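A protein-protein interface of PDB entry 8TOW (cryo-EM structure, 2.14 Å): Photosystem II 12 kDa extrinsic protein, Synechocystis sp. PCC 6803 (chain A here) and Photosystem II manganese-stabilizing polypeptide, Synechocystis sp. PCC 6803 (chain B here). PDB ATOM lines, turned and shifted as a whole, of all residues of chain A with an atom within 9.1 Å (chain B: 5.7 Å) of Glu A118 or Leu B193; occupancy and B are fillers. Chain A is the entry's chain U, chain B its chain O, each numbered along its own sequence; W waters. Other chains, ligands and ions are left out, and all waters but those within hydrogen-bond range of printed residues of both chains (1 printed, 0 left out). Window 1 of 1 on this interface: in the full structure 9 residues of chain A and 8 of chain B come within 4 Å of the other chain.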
ATOM      1  N   LEU A  38      -6.380  12.520  16.613  1.00  0.00           N
ATOM      2  CA  LEU A  38      -5.952  11.971  15.333  1.00  0.00           C
ATOM      3  C   LEU A  38      -6.826  12.484  14.199  1.00  0.00           C
ATOM      4  O   LEU A  38      -8.024  12.717  14.375  1.00  0.00           O
ATOM      5  CB  LEU A  38      -6.032  10.446  15.375  1.00  0.00           C
ATOM      6  CG  LEU A  38      -5.252   9.681  16.438  1.00  0.00           C
ATOM      7  CD1 LEU A  38      -5.567   8.206  16.326  1.00  0.00           C
ATOM      8  CD2 LEU A  38      -3.757   9.922  16.304  1.00  0.00           C
ATOM      9  N   ASN A  39      -6.230  12.635  13.017  1.00  0.00           N
ATOM     10  CA  ASN A  39      -7.047  12.904  11.845  1.00  0.00           C
ATOM     11  C   ASN A  39      -7.636  11.593  11.324  1.00  0.00           C
ATOM     12  O   ASN A  39      -7.574  10.549  11.977  1.00  0.00           O
ATOM     13  CB  ASN A  39      -6.255  13.668  10.777  1.00  0.00           C
ATOM     14  CG  ASN A  39      -4.943  13.004  10.394  1.00  0.00           C
ATOM     15  OD1 ASN A  39      -4.887  11.817  10.075  1.00  0.00           O
ATOM     16  ND2 ASN A  39      -3.876  13.791  10.395  1.00  0.00           N
ATOM     17  N   ALA A  40      -8.209  11.641  10.123  1.00  0.00           N
ATOM     18  CA  ALA A  40      -8.999  10.514   9.637  1.00  0.00           C
ATOM     19  C   ALA A  40      -8.130   9.325   9.231  1.00  0.00           C
ATOM     20  O   ALA A  40      -8.429   8.183   9.598  1.00  0.00           O
ATOM     21  CB  ALA A  40      -9.878  10.960   8.476  1.00  0.00           C
ATOM     22  N   VAL A  41      -7.051   9.560   8.476  1.00  0.00           N
ATOM     23  CA  VAL A  41      -6.264   8.420   8.002  1.00  0.00           C
ATOM     24  C   VAL A  41      -5.379   7.875   9.116  1.00  0.00           C
ATOM     25  O   VAL A  41      -4.996   6.704   9.091  1.00  0.00           O
ATOM     26  CB  VAL A  41      -5.452   8.768   6.738  1.00  0.00           C
ATOM     27  CG1 VAL A  41      -6.289   9.560   5.753  1.00  0.00           C
ATOM     28  CG2 VAL A  41      -4.171   9.495   7.084  1.00  0.00           C
ATOM     29  N   ASP A  42      -5.090   8.684  10.138  1.00  0.00           N
ATOM     30  CA  ASP A  42      -4.410   8.147  11.314  1.00  0.00           C
ATOM     31  C   ASP A  42      -5.331   7.210  12.086  1.00  0.00           C
ATOM     32  O   ASP A  42      -4.906   6.136  12.542  1.00  0.00           O
ATOM     33  CB  ASP A  42      -3.908   9.288  12.198  1.00  0.00           C
ATOM     34  CG  ASP A  42      -2.621   9.902  11.674  1.00  0.00           C
ATOM     35  OD1 ASP A  42      -2.064   9.364  10.695  1.00  0.00           O
ATOM     36  OD2 ASP A  42      -2.161  10.916  12.243  1.00  0.00           O
ATOM     37  N   ALA A  43      -6.612   7.579  12.183  1.00  0.00           N
ATOM     38  CA  ALA A  43      -7.612   6.688  12.759  1.00  0.00           C
ATOM     39  C   ALA A  43      -7.789   5.432  11.913  1.00  0.00           C
ATOM     40  O   ALA A  43      -8.061   4.353  12.448  1.00  0.00           O
ATOM     41  CB  ALA A  43      -8.939   7.428  12.912  1.00  0.00           C
ATOM     42  N   LYS A  44      -7.634   5.554  10.590  1.00  0.00           N
ATOM     43  CA  LYS A  44      -7.689   4.380   9.718  1.00  0.00           C
ATOM     44  C   LYS A  44      -6.491   3.464   9.925  1.00  0.00           C
ATOM     45  O   LYS A  44      -6.627   2.236   9.913  1.00  0.00           O
ATOM     46  CB  LYS A  44      -7.745   4.804   8.253  1.00  0.00           C
ATOM     47  CG  LYS A  44      -9.033   5.433   7.824  1.00  0.00           C
ATOM     48  CD  LYS A  44      -9.217   5.240   6.344  1.00  0.00           C
ATOM     49  CE  LYS A  44      -9.731   3.849   6.039  1.00  0.00           C
ATOM     50  NZ  LYS A  44     -10.976   3.551   6.796  1.00  0.00           N
ATOM     51  N   LEU A  45      -5.301   4.052  10.068  1.00  0.00           N
ATOM     52  CA  LEU A  45      -4.085   3.279  10.290  1.00  0.00           C
ATOM     53  C   LEU A  45      -4.105   2.587  11.644  1.00  0.00           C
ATOM     54  O   LEU A  45      -3.395   1.597  11.842  1.00  0.00           O
ATOM     55  CB  LEU A  45      -2.861   4.190  10.177  1.00  0.00           C
ATOM     56  CG  LEU A  45      -2.451   4.632   8.771  1.00  0.00           C
ATOM     57  CD1 LEU A  45      -1.243   5.552   8.823  1.00  0.00           C
ATOM     58  CD2 LEU A  45      -2.184   3.440   7.872  1.00  0.00           C
ATOM     59  N   PHE A  49      -6.698  -1.069   8.177  1.00  0.00           N
ATOM     60  CA  PHE A  49      -6.148  -0.436   6.986  1.00  0.00           C
ATOM     61  C   PHE A  49      -4.624  -0.386   7.030  1.00  0.00           C
ATOM     62  O   PHE A  49      -3.973  -0.415   5.980  1.00  0.00           O
ATOM     63  CB  PHE A  49      -6.747   0.964   6.848  1.00  0.00           C
ATOM     64  CG  PHE A  49      -6.174   1.768   5.730  1.00  0.00           C
ATOM     65  CD1 PHE A  49      -6.487   1.463   4.418  1.00  0.00           C
ATOM     66  CD2 PHE A  49      -5.332   2.842   5.989  1.00  0.00           C
ATOM     67  CE1 PHE A  49      -5.968   2.205   3.380  1.00  0.00           C
ATOM     68  CE2 PHE A  49      -4.806   3.589   4.951  1.00  0.00           C
ATOM     69  CZ  PHE A  49      -5.130   3.267   3.642  1.00  0.00           C
ATOM     70  N   ASN A  56     -11.438  -0.830  -0.259  1.00  0.00           N
ATOM     71  CA  ASN A  56     -12.176   0.414  -0.402  1.00  0.00           C
ATOM     72  C   ASN A  56     -11.298   1.655  -0.376  1.00  0.00           C
ATOM     73  O   ASN A  56     -11.703   2.685  -0.924  1.00  0.00           O
ATOM     74  CB  ASN A  56     -13.227   0.538   0.707  1.00  0.00           C
ATOM     75  CG  ASN A  56     -14.340  -0.470   0.566  1.00  0.00           C
ATOM     76  OD1 ASN A  56     -15.087  -0.720   1.506  1.00  0.00           O
ATOM     77  ND2 ASN A  56     -14.454  -1.061  -0.616  1.00  0.00           N
ATOM     78  N   ASN A  57     -10.116   1.587   0.233  1.00  0.00           N
ATOM     79  CA  ASN A  57      -9.331   2.787   0.503  1.00  0.00           C
ATOM     80  C   ASN A  57      -7.890   2.727   0.034  1.00  0.00           C
ATOM     81  O   ASN A  57      -7.302   3.790  -0.202  1.00  0.00           O
ATOM     82  CB  ASN A  57      -9.329   3.091   2.007  1.00  0.00           C
ATOM     83  CG  ASN A  57     -10.698   3.430   2.531  1.00  0.00           C
ATOM     84  OD1 ASN A  57     -11.236   4.495   2.239  1.00  0.00           O
ATOM     85  ND2 ASN A  57     -11.277   2.522   3.305  1.00  0.00           N
ATOM     86  N   ASP A  59      -4.434   2.376  -2.081  1.00  0.00           N
ATOM     87  CA  ASP A  59      -4.052   2.806  -3.416  1.00  0.00           C
ATOM     88  C   ASP A  59      -3.706   1.608  -4.295  1.00  0.00           C
ATOM     89  O   ASP A  59      -3.628   0.463  -3.845  1.00  0.00           O
ATOM     90  CB  ASP A  59      -2.859   3.755  -3.368  1.00  0.00           C
ATOM     91  CG  ASP A  59      -2.877   4.647  -2.160  1.00  0.00           C
ATOM     92  OD1 ASP A  59      -3.809   5.470  -2.044  1.00  0.00           O
ATOM     93  OD2 ASP A  59      -1.957   4.519  -1.325  1.00  0.00           O
ATOM     94  N   GLU A 114     -14.741   1.080   6.200  1.00  0.00           N
ATOM     95  CA  GLU A 114     -15.629   2.079   5.631  1.00  0.00           C
ATOM     96  C   GLU A 114     -14.857   2.898   4.602  1.00  0.00           C
ATOM     97  O   GLU A 114     -13.703   3.273   4.863  1.00  0.00           O
ATOM     98  CB  GLU A 114     -16.193   2.992   6.715  1.00  0.00           C
ATOM     99  CG  GLU A 114     -17.256   3.949   6.208  1.00  0.00           C
ATOM    100  CD  GLU A 114     -18.528   3.233   5.802  1.00  0.00           C
ATOM    101  OE1 GLU A 114     -18.877   2.229   6.459  1.00  0.00           O
ATOM    102  OE2 GLU A 114     -19.185   3.678   4.835  1.00  0.00           O
ATOM    103  N   PRO A 115     -15.416   3.135   3.414  1.00  0.00           N
ATOM    104  CA  PRO A 115     -14.719   3.965   2.420  1.00  0.00           C
ATOM    105  C   PRO A 115     -14.569   5.393   2.911  1.00  0.00           C
ATOM    106  O   PRO A 115     -15.549   6.070   3.228  1.00  0.00           O
ATOM    107  CB  PRO A 115     -15.617   3.872   1.178  1.00  0.00           C
ATOM    108  CG  PRO A 115     -16.909   3.319   1.651  1.00  0.00           C
ATOM    109  CD  PRO A 115     -16.607   2.483   2.848  1.00  0.00           C
ATOM    110  N   SER A 116     -13.323   5.835   3.000  1.00  0.00           N
ATOM    111  CA  SER A 116     -12.992   7.141   3.546  1.00  0.00           C
ATOM    112  C   SER A 116     -12.733   8.096   2.392  1.00  0.00           C
ATOM    113  O   SER A 116     -12.024   7.755   1.440  1.00  0.00           O
ATOM    114  CB  SER A 116     -11.786   7.054   4.478  1.00  0.00           C
ATOM    115  OG  SER A 116     -10.576   6.926   3.755  1.00  0.00           O
ATOM    116  N   ILE A 117     -13.318   9.290   2.480  1.00  0.00           N
ATOM    117  CA  ILE A 117     -13.276  10.226   1.370  1.00  0.00           C
ATOM    118  C   ILE A 117     -11.924  10.930   1.310  1.00  0.00           C
ATOM    119  O   ILE A 117     -11.551  11.483   0.268  1.00  0.00           O
ATOM    120  CB  ILE A 117     -14.481  11.181   1.515  1.00  0.00           C
ATOM    121  CG1 ILE A 117     -14.729  11.963   0.231  1.00  0.00           C
ATOM    122  CG2 ILE A 117     -14.275  12.137   2.682  1.00  0.00           C
ATOM    123  CD1 ILE A 117     -16.142  11.983  -0.196  1.00  0.00           C
ATOM    124  N   GLU A 118     -11.158  10.870   2.402  1.00  0.00           N
ATOM    125  CA  GLU A 118      -9.840  11.490   2.465  1.00  0.00           C
ATOM    126  C   GLU A 118      -8.846  10.777   1.561  1.00  0.00           C
ATOM    127  O   GLU A 118      -7.897  11.396   1.072  1.00  0.00           O
ATOM    128  CB  GLU A 118      -9.325  11.483   3.906  1.00  0.00           C
ATOM    129  CG  GLU A 118     -10.142  12.283   4.911  1.00  0.00           C
ATOM    130  CD  GLU A 118     -11.377  11.545   5.401  1.00  0.00           C
ATOM    131  OE1 GLU A 118     -11.309  10.305   5.531  1.00  0.00           O
ATOM    132  OE2 GLU A 118     -12.399  12.204   5.674  1.00  0.00           O
ATOM    133  N   LEU A 119      -9.050   9.483   1.326  1.00  0.00           N
ATOM    134  CA  LEU A 119      -8.195   8.709   0.441  1.00  0.00           C
ATOM    135  C   LEU A 119      -8.794   8.478  -0.939  1.00  0.00           C
ATOM    136  O   LEU A 119      -8.137   7.860  -1.782  1.00  0.00           O
ATOM    137  CB  LEU A 119      -7.871   7.354   1.082  1.00  0.00           C
ATOM    138  CG  LEU A 119      -7.284   7.459   2.486  1.00  0.00           C
ATOM    139  CD1 LEU A 119      -7.336   6.120   3.191  1.00  0.00           C
ATOM    140  CD2 LEU A 119      -5.860   7.968   2.394  1.00  0.00           C
ATOM    141  N   THR A 120     -10.007   8.963  -1.198  1.00  0.00           N
ATOM    142  CA  THR A 120     -10.722   8.624  -2.421  1.00  0.00           C
ATOM    143  C   THR A 120     -10.965   9.819  -3.340  1.00  0.00           C
ATOM    144  O   THR A 120     -10.986   9.642  -4.563  1.00  0.00           O
ATOM    145  CB  THR A 120     -12.055   7.943  -2.058  1.00  0.00           C
ATOM    146  OG1 THR A 120     -11.793   6.874  -1.141  1.00  0.00           O
ATOM    147  CG2 THR A 120     -12.738   7.318  -3.276  1.00  0.00           C
ATOM    148  N   SER A 121     -11.083  11.033  -2.789  1.00  0.00           N
ATOM    149  CA  SER A 121     -11.398  12.220  -3.580  1.00  0.00           C
ATOM    150  C   SER A 121     -10.287  12.556  -4.568  1.00  0.00           C
ATOM    151  O   SER A 121      -9.106  12.517  -4.229  1.00  0.00           O
ATOM    152  CB  SER A 121     -11.615  13.432  -2.675  1.00  0.00           C
ATOM    153  OG  SER A 121     -12.274  13.079  -1.483  1.00  0.00           O
ATOM    154  N   GLY A 122     -10.674  12.906  -5.792  1.00  0.00           N
ATOM    155  CA  GLY A 122      -9.688  13.288  -6.782  1.00  0.00           C
ATOM    156  C   GLY A 122      -8.795  12.164  -7.247  1.00  0.00           C
ATOM    157  O   GLY A 122      -7.656  12.426  -7.648  1.00  0.00           O
ATOM    158  N   ASP A 123      -9.287  10.921  -7.170  1.00  0.00           N
ATOM    159  CA  ASP A 123      -8.612   9.715  -7.661  1.00  0.00           C
ATOM    160  C   ASP A 123      -7.258   9.495  -6.988  1.00  0.00           C
ATOM    161  O   ASP A 123      -6.276   9.141  -7.643  1.00  0.00           O
ATOM    162  CB  ASP A 123      -8.471   9.745  -9.187  1.00  0.00           C
ATOM    163  CG  ASP A 123      -9.710   9.248  -9.895  1.00  0.00           C
ATOM    164  OD1 ASP A 123     -10.038   8.052  -9.750  1.00  0.00           O
ATOM    165  OD2 ASP A 123     -10.367  10.055 -10.589  1.00  0.00           O
ATOM    166  N   ASP A 124      -7.201   9.699  -5.664  1.00  0.00           N
ATOM    167  CA  ASP A 124      -5.970   9.406  -4.932  1.00  0.00           C
ATOM    168  C   ASP A 124      -5.676   7.916  -4.840  1.00  0.00           C
ATOM    169  O   ASP A 124      -4.539   7.544  -4.539  1.00  0.00           O
ATOM    170  CB  ASP A 124      -5.991   9.971  -3.510  1.00  0.00           C
ATOM    171  CG  ASP A 124      -6.082  11.479  -3.466  1.00  0.00           C
ATOM    172  OD1 ASP A 124      -5.297  12.150  -4.168  1.00  0.00           O
ATOM    173  OD2 ASP A 124      -6.864  11.994  -2.644  1.00  0.00           O
ATOM    174  N   ARG A 125      -6.669   7.056  -5.073  1.00  0.00           N
ATOM    175  CA  ARG A 125      -6.410   5.623  -5.101  1.00  0.00           C
ATOM    176  C   ARG A 125      -5.591   5.214  -6.317  1.00  0.00           C
ATOM    177  O   ARG A 125      -4.939   4.167  -6.291  1.00  0.00           O
ATOM    178  CB  ARG A 125      -7.730   4.860  -5.065  1.00  0.00           C
ATOM    179  CG  ARG A 125      -8.530   5.127  -3.803  1.00  0.00           C
ATOM    180  CD  ARG A 125      -9.564   4.053  -3.578  1.00  0.00           C
ATOM    181  NE  ARG A 125      -8.942   2.770  -3.285  1.00  0.00           N
ATOM    182  CZ  ARG A 125      -9.582   1.610  -3.296  1.00  0.00           C
ATOM    183  NH1 ARG A 125     -10.870   1.534  -3.588  1.00  0.00           N
ATOM    184  NH2 ARG A 125      -8.914   0.498  -3.011  1.00  0.00           N
ATOM    185  N   PRO A 128      -1.867   9.054  -5.551  1.00  0.00           N
ATOM    186  CA  PRO A 128      -1.883   9.889  -4.341  1.00  0.00           C
ATOM    187  C   PRO A 128      -0.713  10.852  -4.202  1.00  0.00           C
ATOM    188  O   PRO A 128      -0.513  11.382  -3.106  1.00  0.00           O
ATOM    189  CB  PRO A 128      -1.839   8.841  -3.222  1.00  0.00           C
ATOM    190  CG  PRO A 128      -1.091   7.701  -3.808  1.00  0.00           C
ATOM    191  CD  PRO A 128      -1.266   7.734  -5.303  1.00  0.00           C
ATOM    192  N   ALA B 183      -6.555  16.153   0.588  1.00  0.00           N
ATOM    193  CA  ALA B 183      -5.993  15.705   1.851  1.00  0.00           C
ATOM    194  C   ALA B 183      -4.503  15.383   1.751  1.00  0.00           C
ATOM    195  O   ALA B 183      -3.916  14.925   2.734  1.00  0.00           O
ATOM    196  CB  ALA B 183      -6.801  14.520   2.386  1.00  0.00           C
ATOM    197  N   GLY B 184      -3.882  15.610   0.596  1.00  0.00           N
ATOM    198  CA  GLY B 184      -2.443  15.672   0.458  1.00  0.00           C
ATOM    199  C   GLY B 184      -1.870  17.073   0.462  1.00  0.00           C
ATOM    200  O   GLY B 184      -0.663  17.242   0.278  1.00  0.00           O
ATOM    201  N   PHE B 185      -2.716  18.083   0.650  1.00  0.00           N
ATOM    202  CA  PHE B 185      -2.276  19.469   0.724  1.00  0.00           C
ATOM    203  C   PHE B 185      -1.467  19.698   1.991  1.00  0.00           C
ATOM    204  O   PHE B 185      -1.720  19.078   3.025  1.00  0.00           O
ATOM    205  CB  PHE B 185      -3.491  20.398   0.701  1.00  0.00           C
ATOM    206  CG  PHE B 185      -3.157  21.865   0.612  1.00  0.00           C
ATOM    207  CD1 PHE B 185      -2.806  22.435  -0.599  1.00  0.00           C
ATOM    208  CD2 PHE B 185      -3.226  22.676   1.736  1.00  0.00           C
ATOM    209  CE1 PHE B 185      -2.517  23.789  -0.690  1.00  0.00           C
ATOM    210  CE2 PHE B 185      -2.934  24.022   1.657  1.00  0.00           C
ATOM    211  CZ  PHE B 185      -2.577  24.580   0.440  1.00  0.00           C
ATOM    212  N   ARG B 191       1.676  20.829   7.626  1.00  0.00           N
ATOM    213  CA  ARG B 191       0.674  19.954   8.221  1.00  0.00           C
ATOM    214  C   ARG B 191      -0.407  19.680   7.188  1.00  0.00           C
ATOM    215  O   ARG B 191      -0.930  20.611   6.573  1.00  0.00           O
ATOM    216  CB  ARG B 191       0.041  20.580   9.467  1.00  0.00           C
ATOM    217  CG  ARG B 191       1.019  20.956  10.558  1.00  0.00           C
ATOM    218  CD  ARG B 191       0.324  21.693  11.682  1.00  0.00           C
ATOM    219  NE  ARG B 191      -0.218  22.973  11.241  1.00  0.00           N
ATOM    220  CZ  ARG B 191      -0.604  23.943  12.056  1.00  0.00           C
ATOM    221  NH1 ARG B 191      -0.527  23.813  13.369  1.00  0.00           N
ATOM    222  NH2 ARG B 191      -1.078  25.074  11.541  1.00  0.00           N
ATOM    223  N   GLY B 192      -0.742  18.410   7.007  1.00  0.00           N
ATOM    224  CA  GLY B 192      -1.849  18.039   6.152  1.00  0.00           C
ATOM    225  C   GLY B 192      -2.579  16.844   6.725  1.00  0.00           C
ATOM    226  O   GLY B 192      -2.489  16.596   7.930  1.00  0.00           O
ATOM    227  N   LEU B 193      -3.306  16.094   5.897  1.00  0.00           N
ATOM    228  CA  LEU B 193      -4.086  14.998   6.455  1.00  0.00           C
ATOM    229  C   LEU B 193      -3.370  13.652   6.331  1.00  0.00           C
ATOM    230  O   LEU B 193      -3.017  13.067   7.357  1.00  0.00           O
ATOM    231  CB  LEU B 193      -5.461  14.943   5.797  1.00  0.00           C
ATOM    232  CG  LEU B 193      -6.633  14.483   6.673  1.00  0.00           C
ATOM    233  CD1 LEU B 193      -7.894  14.952   6.035  1.00  0.00           C
ATOM    234  CD2 LEU B 193      -6.716  12.998   6.928  1.00  0.00           C
ATOM    235  N   TYR B 194      -3.124  13.142   5.117  1.00  0.00           N
ATOM    236  CA  TYR B 194      -2.318  11.926   5.052  1.00  0.00           C
ATOM    237  C   TYR B 194      -0.846  12.208   4.828  1.00  0.00           C
ATOM    238  O   TYR B 194      -0.060  11.265   4.713  1.00  0.00           O
ATOM    239  CB  TYR B 194      -2.746  10.928   3.969  1.00  0.00           C
ATOM    240  CG  TYR B 194      -3.127  11.430   2.604  1.00  0.00           C
ATOM    241  CD1 TYR B 194      -2.190  11.415   1.579  1.00  0.00           C
ATOM    242  CD2 TYR B 194      -4.441  11.719   2.279  1.00  0.00           C
ATOM    243  CE1 TYR B 194      -2.515  11.812   0.304  1.00  0.00           C
ATOM    244  CE2 TYR B 194      -4.777  12.088   0.985  1.00  0.00           C
ATOM    245  CZ  TYR B 194      -3.810  12.149   0.012  1.00  0.00           C
ATOM    246  OH  TYR B 194      -4.143  12.533  -1.264  1.00  0.00           O
ATOM    247  N   THR B 195      -0.456  13.466   4.728  1.00  0.00           N
ATOM    248  CA  THR B 195       0.950  13.800   4.660  1.00  0.00           C
ATOM    249  C   THR B 195       1.188  14.951   5.621  1.00  0.00           C
ATOM    250  O   THR B 195       0.259  15.647   6.018  1.00  0.00           O
ATOM    251  CB  THR B 195       1.395  14.126   3.222  1.00  0.00           C
ATOM    252  OG1 THR B 195       2.824  14.129   3.151  1.00  0.00           O
ATOM    253  CG2 THR B 195       0.859  15.464   2.763  1.00  0.00           C
ATOM    254  N   LYS B 215      -6.100  18.095  10.633  1.00  0.00           N
ATOM    255  CA  LYS B 215      -6.777  18.487   9.407  1.00  0.00           C
ATOM    256  C   LYS B 215      -7.957  17.559   9.142  1.00  0.00           C
ATOM    257  O   LYS B 215      -8.041  16.455   9.682  1.00  0.00           O
ATOM    258  CB  LYS B 215      -5.810  18.468   8.221  1.00  0.00           C
ATOM    259  CG  LYS B 215      -4.528  19.258   8.452  1.00  0.00           C
ATOM    260  CD  LYS B 215      -4.805  20.715   8.788  1.00  0.00           C
ATOM    261  CE  LYS B 215      -3.529  21.540   8.708  1.00  0.00           C
ATOM    262  NZ  LYS B 215      -3.712  22.921   9.222  1.00  0.00           N
ATOM    263  N   GLU B 216      -8.876  18.030   8.306  1.00  0.00           N
ATOM    264  CA  GLU B 216     -10.058  17.254   7.957  1.00  0.00           C
ATOM    265  C   GLU B 216     -10.584  17.712   6.604  1.00  0.00           C
ATOM    266  O   GLU B 216     -10.648  18.913   6.333  1.00  0.00           O
ATOM    267  CB  GLU B 216     -11.142  17.372   9.038  1.00  0.00           C
ATOM    268  CG  GLU B 216     -11.350  18.775   9.572  1.00  0.00           C
ATOM    269  CD  GLU B 216     -11.707  18.790  11.050  1.00  0.00           C
ATOM    270  OE1 GLU B 216     -11.693  17.712  11.681  1.00  0.00           O
ATOM    271  OE2 GLU B 216     -11.991  19.885  11.580  1.00  0.00           O
ATOM    272  N   THR B 217     -10.937  16.746   5.752  1.00  0.00           N
ATOM    273  CA  THR B 217     -11.498  17.007   4.421  1.00  0.00           C
ATOM    274  C   THR B 217     -12.847  16.309   4.276  1.00  0.00           C
ATOM    275  O   THR B 217     -12.955  15.268   3.618  1.00  0.00           O
ATOM    276  CB  THR B 217     -10.544  16.566   3.306  1.00  0.00           C
ATOM    277  OG1 THR B 217     -10.449  15.138   3.253  1.00  0.00           O
ATOM    278  CG2 THR B 217      -9.179  17.193   3.437  1.00  0.00           C
ATOM    279  N   PRO B 218     -13.905  16.872   4.857  1.00  0.00           N
ATOM    280  CA  PRO B 218     -15.225  16.244   4.758  1.00  0.00           C
ATOM    281  C   PRO B 218     -15.940  16.602   3.462  1.00  0.00           C
ATOM    282  O   PRO B 218     -15.529  17.486   2.709  1.00  0.00           O
ATOM    283  CB  PRO B 218     -15.969  16.812   5.968  1.00  0.00           C
ATOM    284  CG  PRO B 218     -15.382  18.165   6.145  1.00  0.00           C
ATOM    285  CD  PRO B 218     -13.949  18.093   5.684  1.00  0.00           C
ATOM    286  N   LEU B 252      -8.933  22.926   5.176  1.00  0.00           N
ATOM    287  CA  LEU B 252      -8.757  21.646   5.873  1.00  0.00           C
ATOM    288  C   LEU B 252      -9.379  21.654   7.268  1.00  0.00           C
ATOM    289  O   LEU B 252      -8.864  21.015   8.187  1.00  0.00           O
ATOM    290  CB  LEU B 252      -7.279  21.237   5.950  1.00  0.00           C
ATOM    291  CG  LEU B 252      -6.451  21.182   4.664  1.00  0.00           C
ATOM    292  CD1 LEU B 252      -4.975  21.063   4.993  1.00  0.00           C
ATOM    293  CD2 LEU B 252      -6.882  20.017   3.823  1.00  0.00           C
HETATM  294  O   HOH W   1      -3.680  16.652  10.855  1.00  0.00           O
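Of the 13 printed residues of chain B, 6 touch a printed residue of chain A. Hydrophobic or aromatic side chains of chain B within 4 Å of the printed part of chain A: Ala B183, Leu B193 and Tyr B194. Printed residues of chain A that touch a printed residue of chain B: Asn A39, Ala A40, Val A41, Ile A117, Glu A118, Asp A124 and Pro A128. Among the printed residues, no Asp or Glu carboxylate lies within 4 Å of a Lys or Arg side-chain nitrogen of the other chain.
The side-chain hydroxyl (OH) of Tyr B194 lies within hydrogen-bond range of the side-chain carboxylate (OD2) of Asp A124 (3.1 Å). The backbone carbonyl oxygen of Leu B193 lies within hydrogen-bond range of the side-chain amide nitrogen of Asn A39, at 3.2 Å.
The side-chain amide oxygen (OD1) of Asn A39 is in hydrogen-bond range of the backbone NH (N) of Asp A42 (3.1 Å). The backbone carbonyl oxygen (O) of Ile A117 lies within hydrogen-bond range of the side-chain hydroxyl (OG) of Ser A121, 2.5 Å away. The backbone carbonyl oxygen of Ala B183 lies within hydrogen-bond range of the backbone NH of Leu B193 (3.4 Å). The backbone carbonyl oxygen (O) of Ala B183 lies within hydrogen-bond range of the backbone NH (N) of Tyr B194.
Among the printed residues, pairs that only touch across the chains: Asn A39 with Gly B192 (3.98 Å), Asn A39 with Lys B215 (3.5 Å), Ala A40 with Leu B193 (3.8 Å), Val A41 with Leu B193 (3.7 Å), Val A41 with Tyr B194 (3.7 Å), Ile A117 with Thr B217 (3.5 Å), Glu A118 with Ala B183 (3.6 Å), Glu A118 with Leu B193 (3.7 Å), Glu A118 with Tyr B194 (3.2 Å), Glu A118 with Thr B217 (3.3 Å) and Pro A128 with Tyr B194 (3.98 Å).
Ala A43 touches none of the printed residues of chain B. Leu A45 touches none of the printed residues of chain B. Glu A118 touches four residues of chain B. Printed residues of chain B within 4 Å of Asp A124: Tyr B194. Printed residues of chain B within 4 Å of Pro A128: Tyr B194 (3.98 Å). Leu B193 touches just these residues of chain A: Asn A39, Ala A40, Val A41 and Glu A118. Printed residues of chain A within 4 Å of Tyr B194: Val A41, Glu A118, Asp A124 and Pro A128. Of the printed residues of chain A, Lys B215 touches Asn A39 (3.5 Å). Thr B217 touches two residues of chain A.
Water W1 lies within hydrogen-bond range of N of Lys B215 (2.8 Å), ND2 of Asn A39 (2.9 Å) and O of Gly B192 (3.2 Å).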
